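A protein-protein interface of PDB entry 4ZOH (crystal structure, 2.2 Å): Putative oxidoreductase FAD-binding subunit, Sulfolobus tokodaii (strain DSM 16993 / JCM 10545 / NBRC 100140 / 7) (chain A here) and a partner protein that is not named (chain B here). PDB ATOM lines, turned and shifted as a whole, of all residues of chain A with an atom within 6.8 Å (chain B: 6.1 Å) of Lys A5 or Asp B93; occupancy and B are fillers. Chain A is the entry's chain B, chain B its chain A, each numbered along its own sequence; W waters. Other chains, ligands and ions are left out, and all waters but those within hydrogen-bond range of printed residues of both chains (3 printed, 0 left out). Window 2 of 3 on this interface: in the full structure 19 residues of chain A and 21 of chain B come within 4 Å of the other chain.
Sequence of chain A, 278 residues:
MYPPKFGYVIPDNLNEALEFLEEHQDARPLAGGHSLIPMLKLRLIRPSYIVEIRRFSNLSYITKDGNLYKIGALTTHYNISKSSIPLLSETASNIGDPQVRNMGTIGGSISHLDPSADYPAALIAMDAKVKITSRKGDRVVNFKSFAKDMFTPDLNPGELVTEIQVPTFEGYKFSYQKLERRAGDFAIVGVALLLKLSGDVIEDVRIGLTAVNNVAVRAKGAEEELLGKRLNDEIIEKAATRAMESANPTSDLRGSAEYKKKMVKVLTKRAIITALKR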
ATOM      1  N   TYR A   2      -1.787  21.981  14.281  1.00  0.00           N
ATOM      2  CA  TYR A   2      -2.732  22.599  13.340  1.00  0.00           C
ATOM      3  C   TYR A   2      -3.252  21.437  12.533  1.00  0.00           C
ATOM      4  O   TYR A   2      -2.455  20.769  11.915  1.00  0.00           O
ATOM      5  CB  TYR A   2      -2.014  23.614  12.438  1.00  0.00           C
ATOM      6  CG  TYR A   2      -1.297  24.623  13.306  1.00  0.00           C
ATOM      7  CD1 TYR A   2      -2.000  25.646  13.970  1.00  0.00           C
ATOM      8  CD2 TYR A   2       0.094  24.522  13.523  1.00  0.00           C
ATOM      9  CE1 TYR A   2      -1.355  26.535  14.823  1.00  0.00           C
ATOM     10  CE2 TYR A   2       0.749  25.418  14.371  1.00  0.00           C
ATOM     11  CZ  TYR A   2       0.003  26.429  15.025  1.00  0.00           C
ATOM     12  OH  TYR A   2       0.652  27.306  15.862  1.00  0.00           O
ATOM     13  N   PRO A   3      -4.572  21.148  12.593  1.00  0.00           N
ATOM     14  CA  PRO A   3      -5.121  20.094  11.711  1.00  0.00           C
ATOM     15  C   PRO A   3      -4.802  20.377  10.222  1.00  0.00           C
ATOM     16  O   PRO A   3      -4.431  21.527   9.875  1.00  0.00           O
ATOM     17  CB  PRO A   3      -6.642  20.204  11.916  1.00  0.00           C
ATOM     18  CG  PRO A   3      -6.784  20.853  13.238  1.00  0.00           C
ATOM     19  CD  PRO A   3      -5.656  21.849  13.294  1.00  0.00           C
ATOM     20  N   PRO A   4      -4.925  19.338   9.374  1.00  0.00           N
ATOM     21  CA  PRO A   4      -4.917  19.555   7.944  1.00  0.00           C
ATOM     22  C   PRO A   4      -6.306  20.065   7.536  1.00  0.00           C
ATOM     23  O   PRO A   4      -7.273  20.010   8.338  1.00  0.00           O
ATOM     24  CB  PRO A   4      -4.633  18.128   7.346  1.00  0.00           C
ATOM     25  CG  PRO A   4      -5.081  17.181   8.395  1.00  0.00           C
ATOM     26  CD  PRO A   4      -5.130  17.907   9.729  1.00  0.00           C
ATOM     27  N   LYS A   5      -6.418  20.562   6.292  1.00  0.00           N
ATOM     28  CA  LYS A   5      -7.735  21.051   5.781  1.00  0.00           C
ATOM     29  C   LYS A   5      -8.635  19.874   5.607  1.00  0.00           C
ATOM     30  O   LYS A   5      -8.184  18.846   5.131  1.00  0.00           O
ATOM     31  CB  LYS A   5      -7.605  21.736   4.422  1.00  0.00           C
ATOM     32  CG  LYS A   5      -6.622  22.891   4.427  1.00  0.00           C
ATOM     33  CD  LYS A   5      -6.855  23.838   3.254  1.00  0.00           C
ATOM     34  CE  LYS A   5      -5.738  24.855   3.312  1.00  0.00           C
ATOM     35  NZ  LYS A   5      -5.822  25.784   2.176  1.00  0.00           N
ATOM     36  N   PHE A   6      -9.915  20.051   5.909  1.00  0.00           N
ATOM     37  CA  PHE A   6     -10.867  19.033   5.690  1.00  0.00           C
ATOM     38  C   PHE A   6     -12.223  19.727   5.556  1.00  0.00           C
ATOM     39  O   PHE A   6     -12.388  20.871   6.011  1.00  0.00           O
ATOM     40  CB  PHE A   6     -10.838  17.992   6.831  1.00  0.00           C
ATOM     41  CG  PHE A   6     -10.989  18.587   8.232  1.00  0.00           C
ATOM     42  CD1 PHE A   6     -12.219  19.084   8.675  1.00  0.00           C
ATOM     43  CD2 PHE A   6      -9.865  18.656   9.104  1.00  0.00           C
ATOM     44  CE1 PHE A   6     -12.330  19.626   9.956  1.00  0.00           C
ATOM     45  CE2 PHE A   6      -9.979  19.173  10.398  1.00  0.00           C
ATOM     46  CZ  PHE A   6     -11.205  19.641  10.829  1.00  0.00           C
ATOM     47  N   GLY A   7     -13.169  19.067   4.884  1.00  0.00           N
ATOM     48  CA  GLY A   7     -14.516  19.545   4.818  1.00  0.00           C
ATOM     49  C   GLY A   7     -15.255  19.141   6.072  1.00  0.00           C
ATOM     50  O   GLY A   7     -14.765  18.336   6.851  1.00  0.00           O
ATOM     51  N   ARG A  43      -1.665  15.432  12.694  1.00  0.00           N
ATOM     52  CA  ARG A  43      -1.789  15.052  11.291  1.00  0.00           C
ATOM     53  C   ARG A  43      -1.542  13.553  11.068  1.00  0.00           C
ATOM     54  O   ARG A  43      -0.989  13.129  10.054  1.00  0.00           O
ATOM     55  CB  ARG A  43      -0.927  15.962  10.384  1.00  0.00           C
ATOM     56  CG  ARG A  43      -1.423  17.423  10.406  1.00  0.00           C
ATOM     57  CD  ARG A  43      -0.791  18.283   9.337  1.00  0.00           C
ATOM     58  NE  ARG A  43      -1.114  19.674   9.656  1.00  0.00           N
ATOM     59  CZ  ARG A  43      -1.057  20.690   8.791  1.00  0.00           C
ATOM     60  NH1 ARG A  43      -0.677  20.489   7.526  1.00  0.00           N
ATOM     61  NH2 ARG A  43      -1.371  21.903   9.204  1.00  0.00           N
ATOM     62  N   ARG A  46      -6.114  12.166   8.008  1.00  0.00           N
ATOM     63  CA  ARG A  46      -6.375  13.193   6.991  1.00  0.00           C
ATOM     64  C   ARG A  46      -7.669  12.872   6.293  1.00  0.00           C
ATOM     65  O   ARG A  46      -7.647  12.506   5.145  1.00  0.00           O
ATOM     66  CB  ARG A  46      -5.273  13.208   5.945  1.00  0.00           C
ATOM     67  CG  ARG A  46      -3.952  13.709   6.467  1.00  0.00           C
ATOM     68  CD  ARG A  46      -2.898  13.670   5.386  1.00  0.00           C
ATOM     69  NE  ARG A  46      -1.611  14.122   5.895  1.00  0.00           N
ATOM     70  CZ  ARG A  46      -1.246  15.396   5.956  1.00  0.00           C
ATOM     71  NH1 ARG A  46      -2.063  16.380   5.559  1.00  0.00           N
ATOM     72  NH2 ARG A  46      -0.058  15.690   6.431  1.00  0.00           N
ATOM     73  N   PRO A  47      -8.808  13.016   6.989  1.00  0.00           N
ATOM     74  CA  PRO A  47     -10.045  12.663   6.351  1.00  0.00           C
ATOM     75  C   PRO A  47     -10.475  13.779   5.399  1.00  0.00           C
ATOM     76  O   PRO A  47      -9.977  14.887   5.505  1.00  0.00           O
ATOM     77  CB  PRO A  47     -11.021  12.539   7.516  1.00  0.00           C
ATOM     78  CG  PRO A  47     -10.428  13.272   8.652  1.00  0.00           C
ATOM     79  CD  PRO A  47      -9.023  13.683   8.288  1.00  0.00           C
ATOM     80  N   SER A  48     -11.394  13.479   4.488  1.00  0.00           N
ATOM     81  CA  SER A  48     -11.895  14.421   3.511  1.00  0.00           C
ATOM     82  C   SER A  48     -12.913  15.287   4.205  1.00  0.00           C
ATOM     83  O   SER A  48     -13.022  16.483   3.925  1.00  0.00           O
ATOM     84  CB  SER A  48     -12.559  13.664   2.360  1.00  0.00           C
ATOM     85  OG  SER A  48     -13.423  12.651   2.874  1.00  0.00           O
ATOM     86  N   ARG B  88      -0.396  30.842  10.923  1.00  0.00           N
ATOM     87  CA  ARG B  88       0.236  29.646  11.472  1.00  0.00           C
ATOM     88  C   ARG B  88      -0.213  28.337  10.812  1.00  0.00           C
ATOM     89  O   ARG B  88       0.622  27.432  10.653  1.00  0.00           O
ATOM     90  CB  ARG B  88       0.067  29.550  12.982  1.00  0.00           C
ATOM     91  CG  ARG B  88      -1.345  29.754  13.509  1.00  0.00           C
ATOM     92  CD  ARG B  88      -1.231  30.163  15.014  1.00  0.00           C
ATOM     93  NE  ARG B  88      -0.739  31.545  15.151  1.00  0.00           N
ATOM     94  CZ  ARG B  88      -0.219  32.012  16.286  1.00  0.00           C
ATOM     95  NH1 ARG B  88      -0.110  31.206  17.380  1.00  0.00           N
ATOM     96  NH2 ARG B  88       0.198  33.259  16.344  1.00  0.00           N
ATOM     97  N   TYR B  89      -1.494  28.243  10.445  1.00  0.00           N
ATOM     98  CA  TYR B  89      -2.050  27.040   9.870  1.00  0.00           C
ATOM     99  C   TYR B  89      -1.410  26.807   8.516  1.00  0.00           C
ATOM    100  O   TYR B  89      -0.996  25.700   8.228  1.00  0.00           O
ATOM    101  CB  TYR B  89      -3.598  27.148   9.733  1.00  0.00           C
ATOM    102  CG  TYR B  89      -4.332  26.961  11.071  1.00  0.00           C
ATOM    103  CD1 TYR B  89      -5.061  25.771  11.336  1.00  0.00           C
ATOM    104  CD2 TYR B  89      -4.299  27.954  12.098  1.00  0.00           C
ATOM    105  CE1 TYR B  89      -5.760  25.607  12.552  1.00  0.00           C
ATOM    106  CE2 TYR B  89      -5.005  27.787  13.302  1.00  0.00           C
ATOM    107  CZ  TYR B  89      -5.717  26.606  13.524  1.00  0.00           C
ATOM    108  OH  TYR B  89      -6.392  26.385  14.709  1.00  0.00           O
ATOM    109  N   GLU B  90      -1.287  27.876   7.722  1.00  0.00           N
ATOM    110  CA  GLU B  90      -0.723  27.784   6.386  1.00  0.00           C
ATOM    111  C   GLU B  90       0.754  27.618   6.444  1.00  0.00           C
ATOM    112  O   GLU B  90       1.308  26.878   5.627  1.00  0.00           O
ATOM    113  CB  GLU B  90      -1.103  28.996   5.526  1.00  0.00           C
ATOM    114  CG  GLU B  90      -2.614  29.027   5.280  1.00  0.00           C
ATOM    115  CD  GLU B  90      -3.064  30.141   4.338  1.00  0.00           C
ATOM    116  OE1 GLU B  90      -2.179  30.825   3.778  1.00  0.00           O
ATOM    117  OE2 GLU B  90      -4.285  30.353   4.150  1.00  0.00           O
ATOM    118  N   ALA B  91       1.398  28.223   7.445  1.00  0.00           N
ATOM    119  CA  ALA B  91       2.835  27.990   7.681  1.00  0.00           C
ATOM    120  C   ALA B  91       3.118  26.499   7.864  1.00  0.00           C
ATOM    121  O   ALA B  91       4.104  25.959   7.305  1.00  0.00           O
ATOM    122  CB  ALA B  91       3.396  28.813   8.841  1.00  0.00           C
ATOM    123  N   TYR B  92       2.250  25.808   8.619  1.00  0.00           N
ATOM    124  CA  TYR B  92       2.551  24.405   8.883  1.00  0.00           C
ATOM    125  C   TYR B  92       2.192  23.528   7.683  1.00  0.00           C
ATOM    126  O   TYR B  92       2.853  22.539   7.473  1.00  0.00           O
ATOM    127  CB  TYR B  92       2.040  23.924  10.249  1.00  0.00           C
ATOM    128  CG  TYR B  92       3.006  24.392  11.375  1.00  0.00           C
ATOM    129  CD1 TYR B  92       2.890  25.710  11.918  1.00  0.00           C
ATOM    130  CD2 TYR B  92       4.035  23.562  11.894  1.00  0.00           C
ATOM    131  CE1 TYR B  92       3.731  26.185  12.935  1.00  0.00           C
ATOM    132  CE2 TYR B  92       4.917  24.037  12.921  1.00  0.00           C
ATOM    133  CZ  TYR B  92       4.743  25.364  13.443  1.00  0.00           C
ATOM    134  OH  TYR B  92       5.522  25.945  14.443  1.00  0.00           O
ATOM    135  N   ASP B  93       1.205  23.929   6.883  1.00  0.00           N
ATOM    136  CA  ASP B  93       0.988  23.312   5.565  1.00  0.00           C
ATOM    137  C   ASP B  93       2.262  23.446   4.747  1.00  0.00           C
ATOM    138  O   ASP B  93       2.762  22.454   4.249  1.00  0.00           O
ATOM    139  CB  ASP B  93      -0.166  23.969   4.792  1.00  0.00           C
ATOM    140  CG  ASP B  93      -1.436  23.808   5.454  1.00  0.00           C
ATOM    141  OD1 ASP B  93      -1.554  22.853   6.246  1.00  0.00           O
ATOM    142  OD2 ASP B  93      -2.357  24.637   5.184  1.00  0.00           O
ATOM    143  N   LEU B  94       2.803  24.673   4.650  1.00  0.00           N
ATOM    144  CA  LEU B  94       3.996  24.917   3.863  1.00  0.00           C
ATOM    145  C   LEU B  94       5.210  24.131   4.316  1.00  0.00           C
ATOM    146  O   LEU B  94       6.052  23.783   3.489  1.00  0.00           O
ATOM    147  CB  LEU B  94       4.294  26.409   3.818  1.00  0.00           C
ATOM    148  CG  LEU B  94       5.390  26.930   2.886  1.00  0.00           C
ATOM    149  CD1 LEU B  94       5.154  26.558   1.426  1.00  0.00           C
ATOM    150  CD2 LEU B  94       5.388  28.429   3.043  1.00  0.00           C
ATOM    151  N   ILE B  95       5.321  23.851   5.629  1.00  0.00           N
ATOM    152  CA  ILE B  95       6.417  23.021   6.156  1.00  0.00           C
ATOM    153  C   ILE B  95       6.486  21.676   5.355  1.00  0.00           C
ATOM    154  O   ILE B  95       7.552  21.228   4.973  1.00  0.00           O
ATOM    155  CB  ILE B  95       6.262  22.711   7.681  1.00  0.00           C
ATOM    156  CG1 ILE B  95       6.572  23.925   8.570  1.00  0.00           C
ATOM    157  CG2 ILE B  95       7.171  21.530   8.096  1.00  0.00           C
ATOM    158  CD1 ILE B  95       8.040  24.225   8.753  1.00  0.00           C
ATOM    159  N   GLU B  96       5.342  21.070   5.099  1.00  0.00           N
ATOM    160  CA  GLU B  96       5.244  19.772   4.425  1.00  0.00           C
ATOM    161  C   GLU B  96       5.713  19.781   2.967  1.00  0.00           C
ATOM    162  O   GLU B  96       5.930  18.717   2.396  1.00  0.00           O
ATOM    163  CB  GLU B  96       3.802  19.327   4.410  1.00  0.00           C
ATOM    164  CG  GLU B  96       3.243  19.057   5.792  1.00  0.00           C
ATOM    165  CD  GLU B  96       1.765  18.745   5.767  1.00  0.00           C
ATOM    166  OE1 GLU B  96       1.075  19.140   4.810  1.00  0.00           O
ATOM    167  OE2 GLU B  96       1.294  18.108   6.714  1.00  0.00           O
ATOM    168  N   SER B  97       5.860  20.968   2.372  1.00  0.00           N
ATOM    169  CA  SER B  97       6.371  21.098   1.007  1.00  0.00           C
ATOM    170  C   SER B  97       7.843  21.267   0.954  1.00  0.00           C
ATOM    171  O   SER B  97       8.387  21.222  -0.146  1.00  0.00           O
ATOM    172  CB  SER B  97       5.768  22.311   0.293  1.00  0.00           C
ATOM    173  OG  SER B  97       4.388  22.101   0.201  1.00  0.00           O
HETATM  174  O   HOH W   1      -0.751  28.407  18.082  1.00  0.00           O
HETATM  175  O   HOH W   2       3.227  26.970  16.575  1.00  0.00           O
HETATM  176  O   HOH W   3      -3.794  20.871   5.085  1.00  0.00           O
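Among the printed residues, pairs that only touch across the chains: Tyr A2 with Arg B88 (3.5 Å), Tyr A2 with Tyr B89 (3.7 Å), Tyr A2 with Tyr B92 (3.3 Å), Pro A3 with Tyr B89 (3.8 Å), Lys A5 with Asp B93 (3.9 Å) and Arg A43 with Tyr B89 (3.9 Å).
The guanidinium group (NH1) of Arg A43 lies within salt-bridge range of the side-chain carboxylate (OE2) of Glu B96, 3.2 Å away. The side-chain carboxylate of Glu B96 lies within salt-bridge range of the guanidinium group of Arg A46 (2.8 Å). The side-chain carboxylate (OD1) of Asp B93 lies within salt-bridge range of the guanidinium group (NH1) of Arg A43 (2.8 Å).
Printed residues of chain B within 4 Å of Tyr A2: Arg B88 (3.5 Å), Tyr B89 (3.7 Å) and Tyr B92 (3.3 Å). Of chain B, only Asp B93 comes within 4 Å of Lys A5. Of the printed residues of chain B, Arg A43 touches Tyr B89 (3.9 Å), Asp B93 (2.8 Å) and Glu B96 (3.2 Å). Glu B90 touches none of the printed residues of chain A. Of the printed residues of chain A, Tyr B92 touches Tyr A2 (3.3 Å). Asp B93 touches just these residues of chain A: Lys A5 and Arg A43. Printed residues of chain A within 4 Å of Glu B96: Arg A43 (3.2 Å) and Arg A46 (2.8 Å).
Water W2 bridges the side-chain hydroxyl of Tyr A2 and the side-chain hydroxyl of Tyr B92. Water W1 bridges OH of Tyr A2 and NH1 of Arg B88. Water W3 bridges N of Lys A5 (2.9 Å) and OD1 of Asp B93 (3.2 Å).
Along chain A the printed residues that touch a printed residue of chain B span positions 2 to 46. Hydrophobic or aromatic side chains of chain B within 4 Å of the printed part of chain A: Tyr B89 and Tyr B92. Among the printed residues, 9 pairs touch across the chains. Among the printed residues, Asp or Glu carboxylates within 4 Å of a Lys or Arg side-chain nitrogen of the other chain: Arg A43 with Asp B93, Arg A43 with Glu B96 and Arg A46 with Glu B96.
The backbone carbonyl oxygen (O) of Tyr A2 is in hydrogen-bond range of the guanidinium group (NE) of Arg A43 (2.8 Å). O of Pro A3 sits at hydrogen-bond distance from NH2 of Arg A43 (3.2 Å).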
